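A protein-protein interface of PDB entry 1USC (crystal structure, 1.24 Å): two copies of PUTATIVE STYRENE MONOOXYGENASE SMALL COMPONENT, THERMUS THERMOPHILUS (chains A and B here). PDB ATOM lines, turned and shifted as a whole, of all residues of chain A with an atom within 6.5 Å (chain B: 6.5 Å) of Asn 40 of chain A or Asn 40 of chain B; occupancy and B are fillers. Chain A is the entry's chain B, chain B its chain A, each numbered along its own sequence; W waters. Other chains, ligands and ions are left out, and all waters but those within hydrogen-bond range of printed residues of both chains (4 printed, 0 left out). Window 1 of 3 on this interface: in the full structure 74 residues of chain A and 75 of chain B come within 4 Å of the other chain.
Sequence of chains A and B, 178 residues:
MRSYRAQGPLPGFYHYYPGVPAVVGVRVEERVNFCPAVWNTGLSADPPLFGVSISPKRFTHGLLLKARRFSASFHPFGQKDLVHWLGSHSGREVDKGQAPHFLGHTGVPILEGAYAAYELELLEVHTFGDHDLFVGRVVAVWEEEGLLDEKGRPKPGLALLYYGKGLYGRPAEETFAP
Hydrophobic or aromatic side chains of chain B that line the printed part of chain A: Tyr 16, Val 20, Trp 39, Phe 50, Phe 74 and Leu 133. Along chain B the printed residues that touch a printed residue of chain A span positions 16 to 133. Hydrophobic or aromatic side chains of chain A within 4 Å of the printed part of chain B: Tyr 16, Val 20, Trp 39, Phe 50, Phe 74 and Leu 133. Among the printed residues, 17 pairs touch across the chains.
Tyr 16 of chain A touches Phe 74 of chain B, and with the chains exchanged Phe 74 of chain A touches Tyr 16 of chain B. Trp 39 of chain A touches Thr 41 of chain B, and with the chains exchanged Thr 41 of chain A touches Trp 39 of chain B. Asn 40 of chain A touches its own counterpart, Asn 40 of chain B. Thr 41 of chain B touches its own counterpart, Thr 41 of chain A. 17 positions are printed for both chains. Of the 17 pairs that touch across the chains among the printed residues, 17 have their exchanged pair printed and touching as well.
The side-chain hydroxyl (OH) of Tyr 16 of chain A is in hydrogen-bond range of the indole nitrogen (NE1) of Trp 39 of chain A, at 3.0 Å. The side-chain amide nitrogen of Asn 40 of chain B sits at hydrogen-bond distance from the backbone carbonyl oxygen of Val 20 of chain B (2.8 Å). The side-chain amide nitrogen (ND2) of Asn 40 of chain B sits close to the backbone NH (N) of Ala 22 of chain B, at 3.5 Å. The backbone carbonyl oxygen (O) of Thr 41 of chain B sits at hydrogen-bond distance from the backbone NH (N) of Gly 51 of chain B (2.9 Å). The backbone NH (N) of Ala 22 of chain A sits close to the side-chain amide nitrogen (ND2) of Asn 40 of chain A, at 3.5 Å. The backbone NH (N) of Ser 53 of chain A lies within hydrogen-bond range of the backbone carbonyl oxygen (O) of Trp 39 of chain A (2.9 Å).
Among the printed residues, merely in contact across the chains: Trp 39 of chain A with Thr 41 of chain B (3.1 Å), Thr 41 of chain A with Trp 39 of chain B (3.1 Å), Gly 42 of chain A with Trp 39 of chain B (3.3 Å), Trp 39 of chain A with Gly 42 of chain B (3.4 Å), Tyr 16 of chain A with Gly 42 of chain B (3.4 Å), Tyr 16 of chain A with Phe 74 of chain B (3.5 Å), Phe 74 of chain A with Tyr 16 of chain B (3.5 Å), Gly 42 of chain A with Tyr 16 of chain B (3.5 Å), Tyr 16 of chain A with Phe 50 of chain B (3.6 Å), Phe 50 of chain A with Tyr 16 of chain B (3.6 Å), Leu 133 of chain A with Leu 133 of chain B (3.7 Å), Thr 41 of chain A with Thr 41 of chain B (3.7 Å), Tyr 16 of chain A with Val 20 of chain B (3.7 Å), Val 20 of chain A with Tyr 16 of chain B (3.8 Å) and Asn 40 of chain A with Asn 40 of chain B (3.96 Å).
The side-chain hydroxyl of Thr 41 of chain B is in hydrogen-bond range of the backbone NH of Asn 40 of chain A, 3.4 Å away. The backbone NH (N) of Asn 40 of chain B lies within hydrogen-bond range of the side-chain hydroxyl (OG1) of Thr 41 of chain A (3.4 Å).
Water W2 lies within hydrogen-bond range of OD1 of Asn 40 of chain B and O of Tyr 16 of chain A. Water W4 lies within hydrogen-bond range of OD1 of Asn 40 of chain A (2.8 Å) and O of Tyr 16 of chain B (2.8 Å). Water W1 lies within hydrogen-bond range of OG1 of Thr 41 of chain A, N of Gly 42 of chain A and O of Val 38 of chain B. Water W3 lies within hydrogen-bond range of OG1 of Thr 41 of chain B (3.2 Å), O of Val 38 of chain A (3.3 Å) and N of Gly 42 of chain B (3.4 Å).
Of the printed residues of chain B, Trp 39 of chain A touches Thr 41 (3.1 Å) and Gly 42 (3.4 Å). Of chain B, only Asn 40 (3.96 Å) and Thr 41 (3.4 Å) come within 4 Å of Asn 40 of chain A. Ala 22 of chain B touches none of the printed residues of chain A. Of chain A, only Asn 40 and Thr 41 come within 4 Å of Asn 40 of chain B. Of the printed residues of chain A, Thr 41 of chain B touches Trp 39 (3.1 Å), Asn 40 (3.4 Å) and Thr 41 (3.7 Å). Printed residues of chain A within 4 Å of Phe 74 of chain B: Tyr 16. The nearest residue of chain A that does not touch Asn 40 of chain B is Tyr 16 of chain A (4.5 Å). The nearest printed residue of chain B that does not touch Gly 42 of chain A is Ser 53 of chain B (4.3 Å).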
ATOM      1  N   TYR A  16      -8.786 -12.183  13.477  1.00  0.00           N
ATOM      2  CA  TYR A  16      -7.547 -11.617  14.003  1.00  0.00           C
ATOM      3  C   TYR A  16      -7.504 -11.516  15.525  1.00  0.00           C
ATOM      4  O   TYR A  16      -6.611 -10.880  16.082  1.00  0.00           O
ATOM      5  CB  TYR A  16      -7.312 -10.232  13.392  1.00  0.00           C
ATOM      6  CG  TYR A  16      -8.502  -9.313  13.484  1.00  0.00           C
ATOM      7  CD1 TYR A  16      -9.545  -9.400  12.566  1.00  0.00           C
ATOM      8  CD2 TYR A  16      -8.597  -8.370  14.503  1.00  0.00           C
ATOM      9  CE1 TYR A  16     -10.653  -8.571  12.659  1.00  0.00           C
ATOM     10  CE2 TYR A  16      -9.700  -7.534  14.606  1.00  0.00           C
ATOM     11  CZ  TYR A  16     -10.725  -7.641  13.681  1.00  0.00           C
ATOM     12  OH  TYR A  16     -11.821  -6.817  13.775  1.00  0.00           O
ATOM     13  N   GLY A  19      -7.223 -10.169  21.272  1.00  0.00           N
ATOM     14  CA  GLY A  19      -6.472  -8.941  21.393  1.00  0.00           C
ATOM     15  C   GLY A  19      -6.614  -8.428  22.808  1.00  0.00           C
ATOM     16  O   GLY A  19      -7.548  -8.800  23.527  1.00  0.00           O
ATOM     17  N   VAL A  20      -5.671  -7.598  23.229  1.00  0.00           N
ATOM     18  CA  VAL A  20      -5.733  -7.003  24.551  1.00  0.00           C
ATOM     19  C   VAL A  20      -6.696  -5.828  24.434  1.00  0.00           C
ATOM     20  O   VAL A  20      -6.581  -5.015  23.513  1.00  0.00           O
ATOM     21  CB  VAL A  20      -4.357  -6.471  24.993  1.00  0.00           C
ATOM     22  CG1 VAL A  20      -4.516  -5.578  26.221  1.00  0.00           C
ATOM     23  CG2 VAL A  20      -3.425  -7.628  25.308  1.00  0.00           C
ATOM     24  N   PRO A  21      -7.681  -5.738  25.334  1.00  0.00           N
ATOM     25  CA  PRO A  21      -8.615  -4.615  25.253  1.00  0.00           C
ATOM     26  C   PRO A  21      -8.061  -3.414  26.014  1.00  0.00           C
ATOM     27  O   PRO A  21      -7.628  -3.545  27.159  1.00  0.00           O
ATOM     28  CB  PRO A  21      -9.880  -5.175  25.892  1.00  0.00           C
ATOM     29  CG  PRO A  21      -9.334  -6.078  26.955  1.00  0.00           C
ATOM     30  CD  PRO A  21      -8.153  -6.761  26.283  1.00  0.00           C
ATOM     31  N   ALA A  22      -8.048  -2.254  25.372  1.00  0.00           N
ATOM     32  CA  ALA A  22      -7.563  -1.047  26.023  1.00  0.00           C
ATOM     33  C   ALA A  22      -8.760  -0.385  26.686  1.00  0.00           C
ATOM     34  O   ALA A  22      -9.768  -0.119  26.028  1.00  0.00           O
ATOM     35  CB  ALA A  22      -6.954  -0.105  24.997  1.00  0.00           C
ATOM     36  N   ALA A  37     -11.846  -1.065  24.437  1.00  0.00           N
ATOM     37  CA  ALA A  37     -11.713  -1.008  22.993  1.00  0.00           C
ATOM     38  C   ALA A  37     -10.700  -2.061  22.575  1.00  0.00           C
ATOM     39  O   ALA A  37      -9.512  -1.899  22.830  1.00  0.00           O
ATOM     40  CB  ALA A  37     -11.244   0.374  22.563  1.00  0.00           C
ATOM     41  N   VAL A  38     -11.164  -3.147  21.954  1.00  0.00           N
ATOM     42  CA  VAL A  38     -10.244  -4.185  21.503  1.00  0.00           C
ATOM     43  C   VAL A  38      -9.631  -3.765  20.165  1.00  0.00           C
ATOM     44  O   VAL A  38      -8.593  -4.289  19.749  1.00  0.00           O
ATOM     45  CB  VAL A  38     -10.943  -5.567  21.380  1.00  0.00           C
ATOM     46  CG1 VAL A  38     -11.899  -5.580  20.200  1.00  0.00           C
ATOM     47  CG2 VAL A  38      -9.896  -6.668  21.263  1.00  0.00           C
ATOM     48  N   TRP A  39     -10.269  -2.810  19.492  1.00  0.00           N
ATOM     49  CA  TRP A  39      -9.713  -2.300  18.252  1.00  0.00           C
ATOM     50  C   TRP A  39      -8.776  -1.168  18.655  1.00  0.00           C
ATOM     51  O   TRP A  39      -9.162   0.003  18.699  1.00  0.00           O
ATOM     52  CB  TRP A  39     -10.810  -1.792  17.315  1.00  0.00           C
ATOM     53  CG  TRP A  39     -11.589  -2.887  16.656  1.00  0.00           C
ATOM     54  CD1 TRP A  39     -11.438  -4.235  16.842  1.00  0.00           C
ATOM     55  CD2 TRP A  39     -12.660  -2.728  15.722  1.00  0.00           C
ATOM     56  NE1 TRP A  39     -12.355  -4.923  16.078  1.00  0.00           N
ATOM     57  CE2 TRP A  39     -13.116  -4.020  15.383  1.00  0.00           C
ATOM     58  CE3 TRP A  39     -13.279  -1.615  15.136  1.00  0.00           C
ATOM     59  CZ2 TRP A  39     -14.168  -4.232  14.485  1.00  0.00           C
ATOM     60  CZ3 TRP A  39     -14.324  -1.824  14.245  1.00  0.00           C
ATOM     61  CH2 TRP A  39     -14.758  -3.124  13.929  1.00  0.00           C
ATOM     62  N   ASN A  40      -7.546  -1.538  18.989  1.00  0.00           N
ATOM     63  CA  ASN A  40      -6.534  -0.573  19.388  1.00  0.00           C
ATOM     64  C   ASN A  40      -5.203  -1.067  18.850  1.00  0.00           C
ATOM     65  O   ASN A  40      -5.043  -2.260  18.559  1.00  0.00           O
ATOM     66  CB  ASN A  40      -6.482  -0.438  20.918  1.00  0.00           C
ATOM     67  CG  ASN A  40      -5.913  -1.665  21.599  1.00  0.00           C
ATOM     68  OD1 ASN A  40      -4.693  -1.852  21.653  1.00  0.00           O
ATOM     69  ND2 ASN A  40      -6.792  -2.518  22.118  1.00  0.00           N
ATOM     70  N   THR A  41      -4.252  -0.156  18.698  1.00  0.00           N
ATOM     71  CA  THR A  41      -2.945  -0.533  18.190  1.00  0.00           C
ATOM     72  C   THR A  41      -1.943   0.598  18.328  1.00  0.00           C
ATOM     73  O   THR A  41      -2.314   1.769  18.421  1.00  0.00           O
ATOM     74  CB  THR A  41      -3.020  -0.907  16.688  1.00  0.00           C
ATOM     75  OG1 THR A  41      -1.713  -1.247  16.210  1.00  0.00           O
ATOM     76  CG2 THR A  41      -3.555   0.259  15.871  1.00  0.00           C
ATOM     77  N   GLY A  42      -0.667   0.233  18.364  1.00  0.00           N
ATOM     78  CA  GLY A  42       0.368   1.243  18.393  1.00  0.00           C
ATOM     79  C   GLY A  42       0.331   1.807  16.981  1.00  0.00           C
ATOM     80  O   GLY A  42      -0.079   1.114  16.042  1.00  0.00           O
ATOM     81  N   PHE A  50      -0.723   6.123  19.871  1.00  0.00           N
ATOM     82  CA  PHE A  50      -1.543   4.948  20.127  1.00  0.00           C
ATOM     83  C   PHE A  50      -2.964   5.264  19.679  1.00  0.00           C
ATOM     84  O   PHE A  50      -3.469   6.354  19.946  1.00  0.00           O
ATOM     85  CB  PHE A  50      -1.514   4.646  21.628  1.00  0.00           C
ATOM     86  CG  PHE A  50      -2.233   3.391  22.015  1.00  0.00           C
ATOM     87  CD1 PHE A  50      -1.678   2.139  21.764  1.00  0.00           C
ATOM     88  CD2 PHE A  50      -3.481   3.460  22.623  1.00  0.00           C
ATOM     89  CE1 PHE A  50      -2.364   0.971  22.115  1.00  0.00           C
ATOM     90  CE2 PHE A  50      -4.170   2.305  22.974  1.00  0.00           C
ATOM     91  CZ  PHE A  50      -3.612   1.059  22.720  1.00  0.00           C
ATOM     92  N   GLY A  51      -3.611   4.321  19.006  1.00  0.00           N
ATOM     93  CA  GLY A  51      -4.959   4.577  18.543  1.00  0.00           C
ATOM     94  C   GLY A  51      -6.019   3.609  19.019  1.00  0.00           C
ATOM     95  O   GLY A  51      -5.740   2.436  19.272  1.00  0.00           O
ATOM     96  N   VAL A  52      -7.236   4.120  19.162  1.00  0.00           N
ATOM     97  CA  VAL A  52      -8.384   3.312  19.557  1.00  0.00           C
ATOM     98  C   VAL A  52      -9.511   3.657  18.587  1.00  0.00           C
ATOM     99  O   VAL A  52      -9.738   4.833  18.270  1.00  0.00           O
ATOM    100  CB  VAL A  52      -8.839   3.590  21.023  1.00  0.00           C
ATOM    101  CG1 VAL A  52      -7.750   3.158  21.992  1.00  0.00           C
ATOM    102  CG2 VAL A  52      -9.182   5.062  21.211  1.00  0.00           C
ATOM    103  N   SER A  53     -10.193   2.628  18.097  1.00  0.00           N
ATOM    104  CA  SER A  53     -11.289   2.799  17.147  1.00  0.00           C
ATOM    105  C   SER A  53     -12.607   2.708  17.903  1.00  0.00           C
ATOM    106  O   SER A  53     -12.967   1.648  18.415  1.00  0.00           O
ATOM    107  CB  SER A  53     -11.204   1.716  16.074  1.00  0.00           C
ATOM    108  OG  SER A  53     -12.219   1.880  15.103  1.00  0.00           O
ATOM    109  N   PHE A  74      -4.355  -0.963  30.670  1.00  0.00           N
ATOM    110  CA  PHE A  74      -4.257  -2.385  30.372  1.00  0.00           C
ATOM    111  C   PHE A  74      -4.302  -3.163  31.680  1.00  0.00           C
ATOM    112  O   PHE A  74      -3.478  -2.957  32.578  1.00  0.00           O
ATOM    113  CB  PHE A  74      -2.967  -2.592  29.581  1.00  0.00           C
ATOM    114  CG  PHE A  74      -2.832  -1.623  28.437  1.00  0.00           C
ATOM    115  CD1 PHE A  74      -3.626  -1.758  27.303  1.00  0.00           C
ATOM    116  CD2 PHE A  74      -1.984  -0.522  28.531  1.00  0.00           C
ATOM    117  CE1 PHE A  74      -3.582  -0.809  26.281  1.00  0.00           C
ATOM    118  CE2 PHE A  74      -1.936   0.433  27.513  1.00  0.00           C
ATOM    119  CZ  PHE A  74      -2.739   0.286  26.390  1.00  0.00           C
ATOM    120  N   LEU A 133     -11.268   6.364  14.216  1.00  0.00           N
ATOM    121  CA  LEU A 133      -9.992   6.083  14.857  1.00  0.00           C
ATOM    122  C   LEU A 133      -9.498   7.338  15.567  1.00  0.00           C
ATOM    123  O   LEU A 133      -9.285   8.375  14.936  1.00  0.00           O
ATOM    124  CB  LEU A 133      -8.952   5.645  13.822  1.00  0.00           C
ATOM    125  CG  LEU A 133      -7.556   5.358  14.386  1.00  0.00           C
ATOM    126  CD1 LEU A 133      -7.606   4.108  15.245  1.00  0.00           C
ATOM    127  CD2 LEU A 133      -6.554   5.182  13.253  1.00  0.00           C
ATOM    128  N   TYR B  16       0.901  -2.437  25.756  1.00  0.00           N
ATOM    129  CA  TYR B  16      -0.352  -2.954  25.216  1.00  0.00           C
ATOM    130  C   TYR B  16      -0.229  -4.313  24.533  1.00  0.00           C
ATOM    131  O   TYR B  16      -1.176  -4.777  23.900  1.00  0.00           O
ATOM    132  CB  TYR B  16      -0.947  -1.943  24.237  1.00  0.00           C
ATOM    133  CG  TYR B  16       0.041  -1.472  23.203  1.00  0.00           C
ATOM    134  CD1 TYR B  16       0.954  -0.461  23.495  1.00  0.00           C
ATOM    135  CD2 TYR B  16       0.093  -2.065  21.943  1.00  0.00           C
ATOM    136  CE1 TYR B  16       1.895  -0.053  22.563  1.00  0.00           C
ATOM    137  CE2 TYR B  16       1.029  -1.665  21.002  1.00  0.00           C
ATOM    138  CZ  TYR B  16       1.928  -0.658  21.319  1.00  0.00           C
ATOM    139  OH  TYR B  16       2.862  -0.259  20.397  1.00  0.00           O
ATOM    140  N   GLY B  19      -0.059  -9.161  21.078  1.00  0.00           N
ATOM    141  CA  GLY B  19      -1.025  -8.992  20.014  1.00  0.00           C
ATOM    142  C   GLY B  19      -0.783 -10.048  18.957  1.00  0.00           C
ATOM    143  O   GLY B  19       0.319 -10.588  18.849  1.00  0.00           O
ATOM    144  N   VAL B  20      -1.819 -10.372  18.196  1.00  0.00           N
ATOM    145  CA  VAL B  20      -1.680 -11.338  17.120  1.00  0.00           C
ATOM    146  C   VAL B  20      -1.042 -10.598  15.951  1.00  0.00           C
ATOM    147  O   VAL B  20      -1.476  -9.506  15.589  1.00  0.00           O
ATOM    148  CB  VAL B  20      -3.050 -11.879  16.666  1.00  0.00           C
ATOM    149  CG1 VAL B  20      -2.892 -12.679  15.378  1.00  0.00           C
ATOM    150  CG2 VAL B  20      -3.650 -12.750  17.757  1.00  0.00           C
ATOM    151  N   PRO B  21       0.021 -11.161  15.371  1.00  0.00           N
ATOM    152  CA  PRO B  21       0.666 -10.498  14.238  1.00  0.00           C
ATOM    153  C   PRO B  21      -0.052 -10.869  12.943  1.00  0.00           C
ATOM    154  O   PRO B  21      -0.366 -12.037  12.710  1.00  0.00           O
ATOM    155  CB  PRO B  21       2.088 -11.040  14.289  1.00  0.00           C
ATOM    156  CG  PRO B  21       1.891 -12.439  14.780  1.00  0.00           C
ATOM    157  CD  PRO B  21       0.825 -12.297  15.856  1.00  0.00           C
ATOM    158  N   ALA B  22      -0.346  -9.871  12.121  1.00  0.00           N
ATOM    159  CA  ALA B  22      -1.001 -10.116  10.846  1.00  0.00           C
ATOM    160  C   ALA B  22       0.104 -10.239   9.812  1.00  0.00           C
ATOM    161  O   ALA B  22       0.935  -9.339   9.684  1.00  0.00           O
ATOM    162  CB  ALA B  22      -1.917  -8.949  10.489  1.00  0.00           C
ATOM    163  N   ALA B  37       2.991  -7.882  10.927  1.00  0.00           N
ATOM    164  CA  ALA B  37       2.663  -6.575  11.463  1.00  0.00           C
ATOM    165  C   ALA B  37       1.841  -6.774  12.731  1.00  0.00           C
ATOM    166  O   ALA B  37       0.689  -7.186  12.655  1.00  0.00           O
ATOM    167  CB  ALA B  37       1.876  -5.776  10.440  1.00  0.00           C
ATOM    168  N   VAL B  38       2.432  -6.515  13.899  1.00  0.00           N
ATOM    169  CA  VAL B  38       1.685  -6.667  15.144  1.00  0.00           C
ATOM    170  C   VAL B  38       0.823  -5.424  15.370  1.00  0.00           C
ATOM    171  O   VAL B  38      -0.123  -5.444  16.164  1.00  0.00           O
ATOM    172  CB  VAL B  38       2.611  -6.916  16.371  1.00  0.00           C
ATOM    173  CG1 VAL B  38       3.389  -5.662  16.722  1.00  0.00           C
ATOM    174  CG2 VAL B  38       1.778  -7.394  17.558  1.00  0.00           C
ATOM    175  N   TRP B  39       1.143  -4.339  14.665  1.00  0.00           N
ATOM    176  CA  TRP B  39       0.322  -3.141  14.776  1.00  0.00           C
ATOM    177  C   TRP B  39      -0.762  -3.278  13.716  1.00  0.00           C
ATOM    178  O   TRP B  39      -0.610  -2.829  12.573  1.00  0.00           O
ATOM    179  CB  TRP B  39       1.143  -1.867  14.547  1.00  0.00           C
ATOM    180  CG  TRP B  39       2.033  -1.499  15.700  1.00  0.00           C
ATOM    181  CD1 TRP B  39       2.205  -2.192  16.866  1.00  0.00           C
ATOM    182  CD2 TRP B  39       2.891  -0.356  15.784  1.00  0.00           C
ATOM    183  NE1 TRP B  39       3.122  -1.551  17.669  1.00  0.00           N
ATOM    184  CE2 TRP B  39       3.556  -0.421  17.028  1.00  0.00           C
ATOM    185  CE3 TRP B  39       3.165   0.718  14.924  1.00  0.00           C
ATOM    186  CZ2 TRP B  39       4.481   0.550  17.436  1.00  0.00           C
ATOM    187  CZ3 TRP B  39       4.086   1.682  15.330  1.00  0.00           C
ATOM    188  CH2 TRP B  39       4.732   1.588  16.575  1.00  0.00           C
ATOM    189  N   ASN B  40      -1.847  -3.944  14.098  1.00  0.00           N
ATOM    190  CA  ASN B  40      -2.974  -4.162  13.208  1.00  0.00           C
ATOM    191  C   ASN B  40      -4.232  -4.112  14.053  1.00  0.00           C
ATOM    192  O   ASN B  40      -4.182  -4.305  15.273  1.00  0.00           O
ATOM    193  CB  ASN B  40      -2.851  -5.519  12.493  1.00  0.00           C
ATOM    194  CG  ASN B  40      -3.020  -6.706  13.430  1.00  0.00           C
ATOM    195  OD1 ASN B  40      -4.140  -7.089  13.770  1.00  0.00           O
ATOM    196  ND2 ASN B  40      -1.905  -7.291  13.856  1.00  0.00           N
ATOM    197  N   THR B  41      -5.360  -3.839  13.413  1.00  0.00           N
ATOM    198  CA  THR B  41      -6.613  -3.749  14.138  1.00  0.00           C
ATOM    199  C   THR B  41      -7.791  -3.658  13.191  1.00  0.00           C
ATOM    200  O   THR B  41      -7.652  -3.259  12.031  1.00  0.00           O
ATOM    201  CB  THR B  41      -6.648  -2.486  15.035  1.00  0.00           C
ATOM    202  OG1 THR B  41      -7.895  -2.430  15.741  1.00  0.00           O
ATOM    203  CG2 THR B  41      -6.508  -1.226  14.184  1.00  0.00           C
ATOM    204  N   GLY B  42      -8.954  -4.053  13.693  1.00  0.00           N
ATOM    205  CA  GLY B  42     -10.158  -3.930  12.904  1.00  0.00           C
ATOM    206  C   GLY B  42     -10.439  -2.440  12.928  1.00  0.00           C
ATOM    207  O   GLY B  42     -10.024  -1.745  13.862  1.00  0.00           O
ATOM    208  N   PHE B  50      -9.931  -3.326   7.743  1.00  0.00           N
ATOM    209  CA  PHE B  50      -8.862  -3.821   8.597  1.00  0.00           C
ATOM    210  C   PHE B  50      -7.607  -3.018   8.284  1.00  0.00           C
ATOM    211  O   PHE B  50      -7.299  -2.772   7.116  1.00  0.00           O
ATOM    212  CB  PHE B  50      -8.637  -5.303   8.287  1.00  0.00           C
ATOM    213  CG  PHE B  50      -7.629  -5.969   9.174  1.00  0.00           C
ATOM    214  CD1 PHE B  50      -7.941  -6.283  10.491  1.00  0.00           C
ATOM    215  CD2 PHE B  50      -6.360  -6.283   8.692  1.00  0.00           C
ATOM    216  CE1 PHE B  50      -7.003  -6.898  11.318  1.00  0.00           C
ATOM    217  CE2 PHE B  50      -5.421  -6.897   9.509  1.00  0.00           C
ATOM    218  CZ  PHE B  50      -5.746  -7.204  10.827  1.00  0.00           C
ATOM    219  N   GLY B  51      -6.874  -2.614   9.315  1.00  0.00           N
ATOM    220  CA  GLY B  51      -5.679  -1.829   9.071  1.00  0.00           C
ATOM    221  C   GLY B  51      -4.389  -2.410   9.610  1.00  0.00           C
ATOM    222  O   GLY B  51      -4.390  -3.136  10.606  1.00  0.00           O
ATOM    223  N   VAL B  52      -3.289  -2.110   8.924  1.00  0.00           N
ATOM    224  CA  VAL B  52      -1.957  -2.536   9.344  1.00  0.00           C
ATOM    225  C   VAL B  52      -1.063  -1.295   9.282  1.00  0.00           C
ATOM    226  O   VAL B  52      -1.138  -0.513   8.327  1.00  0.00           O
ATOM    227  CB  VAL B  52      -1.379  -3.658   8.439  1.00  0.00           C
ATOM    228  CG1 VAL B  52      -2.208  -4.919   8.597  1.00  0.00           C
ATOM    229  CG2 VAL B  52      -1.346  -3.214   6.982  1.00  0.00           C
ATOM    230  N   SER B  53      -0.243  -1.106  10.314  1.00  0.00           N
ATOM    231  CA  SER B  53       0.652   0.047  10.399  1.00  0.00           C
ATOM    232  C   SER B  53       2.056  -0.393  10.013  1.00  0.00           C
ATOM    233  O   SER B  53       2.695  -1.162  10.735  1.00  0.00           O
ATOM    234  CB  SER B  53       0.636   0.603  11.823  1.00  0.00           C
ATOM    235  OG  SER B  53       1.473   1.739  11.935  1.00  0.00           O
ATOM    236  N   PHE B  74      -3.467 -14.975   9.374  1.00  0.00           N
ATOM    237  CA  PHE B  74      -3.292 -15.257  10.792  1.00  0.00           C
ATOM    238  C   PHE B  74      -2.891 -16.712  10.941  1.00  0.00           C
ATOM    239  O   PHE B  74      -3.586 -17.619  10.482  1.00  0.00           O
ATOM    240  CB  PHE B  74      -4.601 -14.901  11.481  1.00  0.00           C
ATOM    241  CG  PHE B  74      -5.089 -13.530  11.100  1.00  0.00           C
ATOM    242  CD1 PHE B  74      -4.440 -12.395  11.576  1.00  0.00           C
ATOM    243  CD2 PHE B  74      -6.110 -13.371  10.168  1.00  0.00           C
ATOM    244  CE1 PHE B  74      -4.795 -11.121  11.121  1.00  0.00           C
ATOM    245  CE2 PHE B  74      -6.471 -12.097   9.709  1.00  0.00           C
ATOM    246  CZ  PHE B  74      -5.808 -10.976  10.186  1.00  0.00           C
ATOM    247  N   LEU B 133      -0.483   4.014   8.316  1.00  0.00           N
ATOM    248  CA  LEU B 133      -1.580   3.080   8.491  1.00  0.00           C
ATOM    249  C   LEU B 133      -2.218   2.806   7.136  1.00  0.00           C
ATOM    250  O   LEU B 133      -2.714   3.723   6.474  1.00  0.00           O
ATOM    251  CB  LEU B 133      -2.637   3.647   9.441  1.00  0.00           C
ATOM    252  CG  LEU B 133      -3.852   2.741   9.665  1.00  0.00           C
ATOM    253  CD1 LEU B 133      -3.431   1.499  10.442  1.00  0.00           C
ATOM    254  CD2 LEU B 133      -4.931   3.506  10.424  1.00  0.00           C
HETATM  255  O   HOH W   1      -0.709  -3.074  18.421  1.00  0.00           O
HETATM  256  O   HOH W   2      -5.095  -8.548  15.908  1.00  0.00           O
HETATM  257  O   HOH W   3      -8.218  -5.426  16.671  1.00  0.00           O
HETATM  258  O   HOH W   4      -3.136  -4.121  21.991  1.00  0.00           O
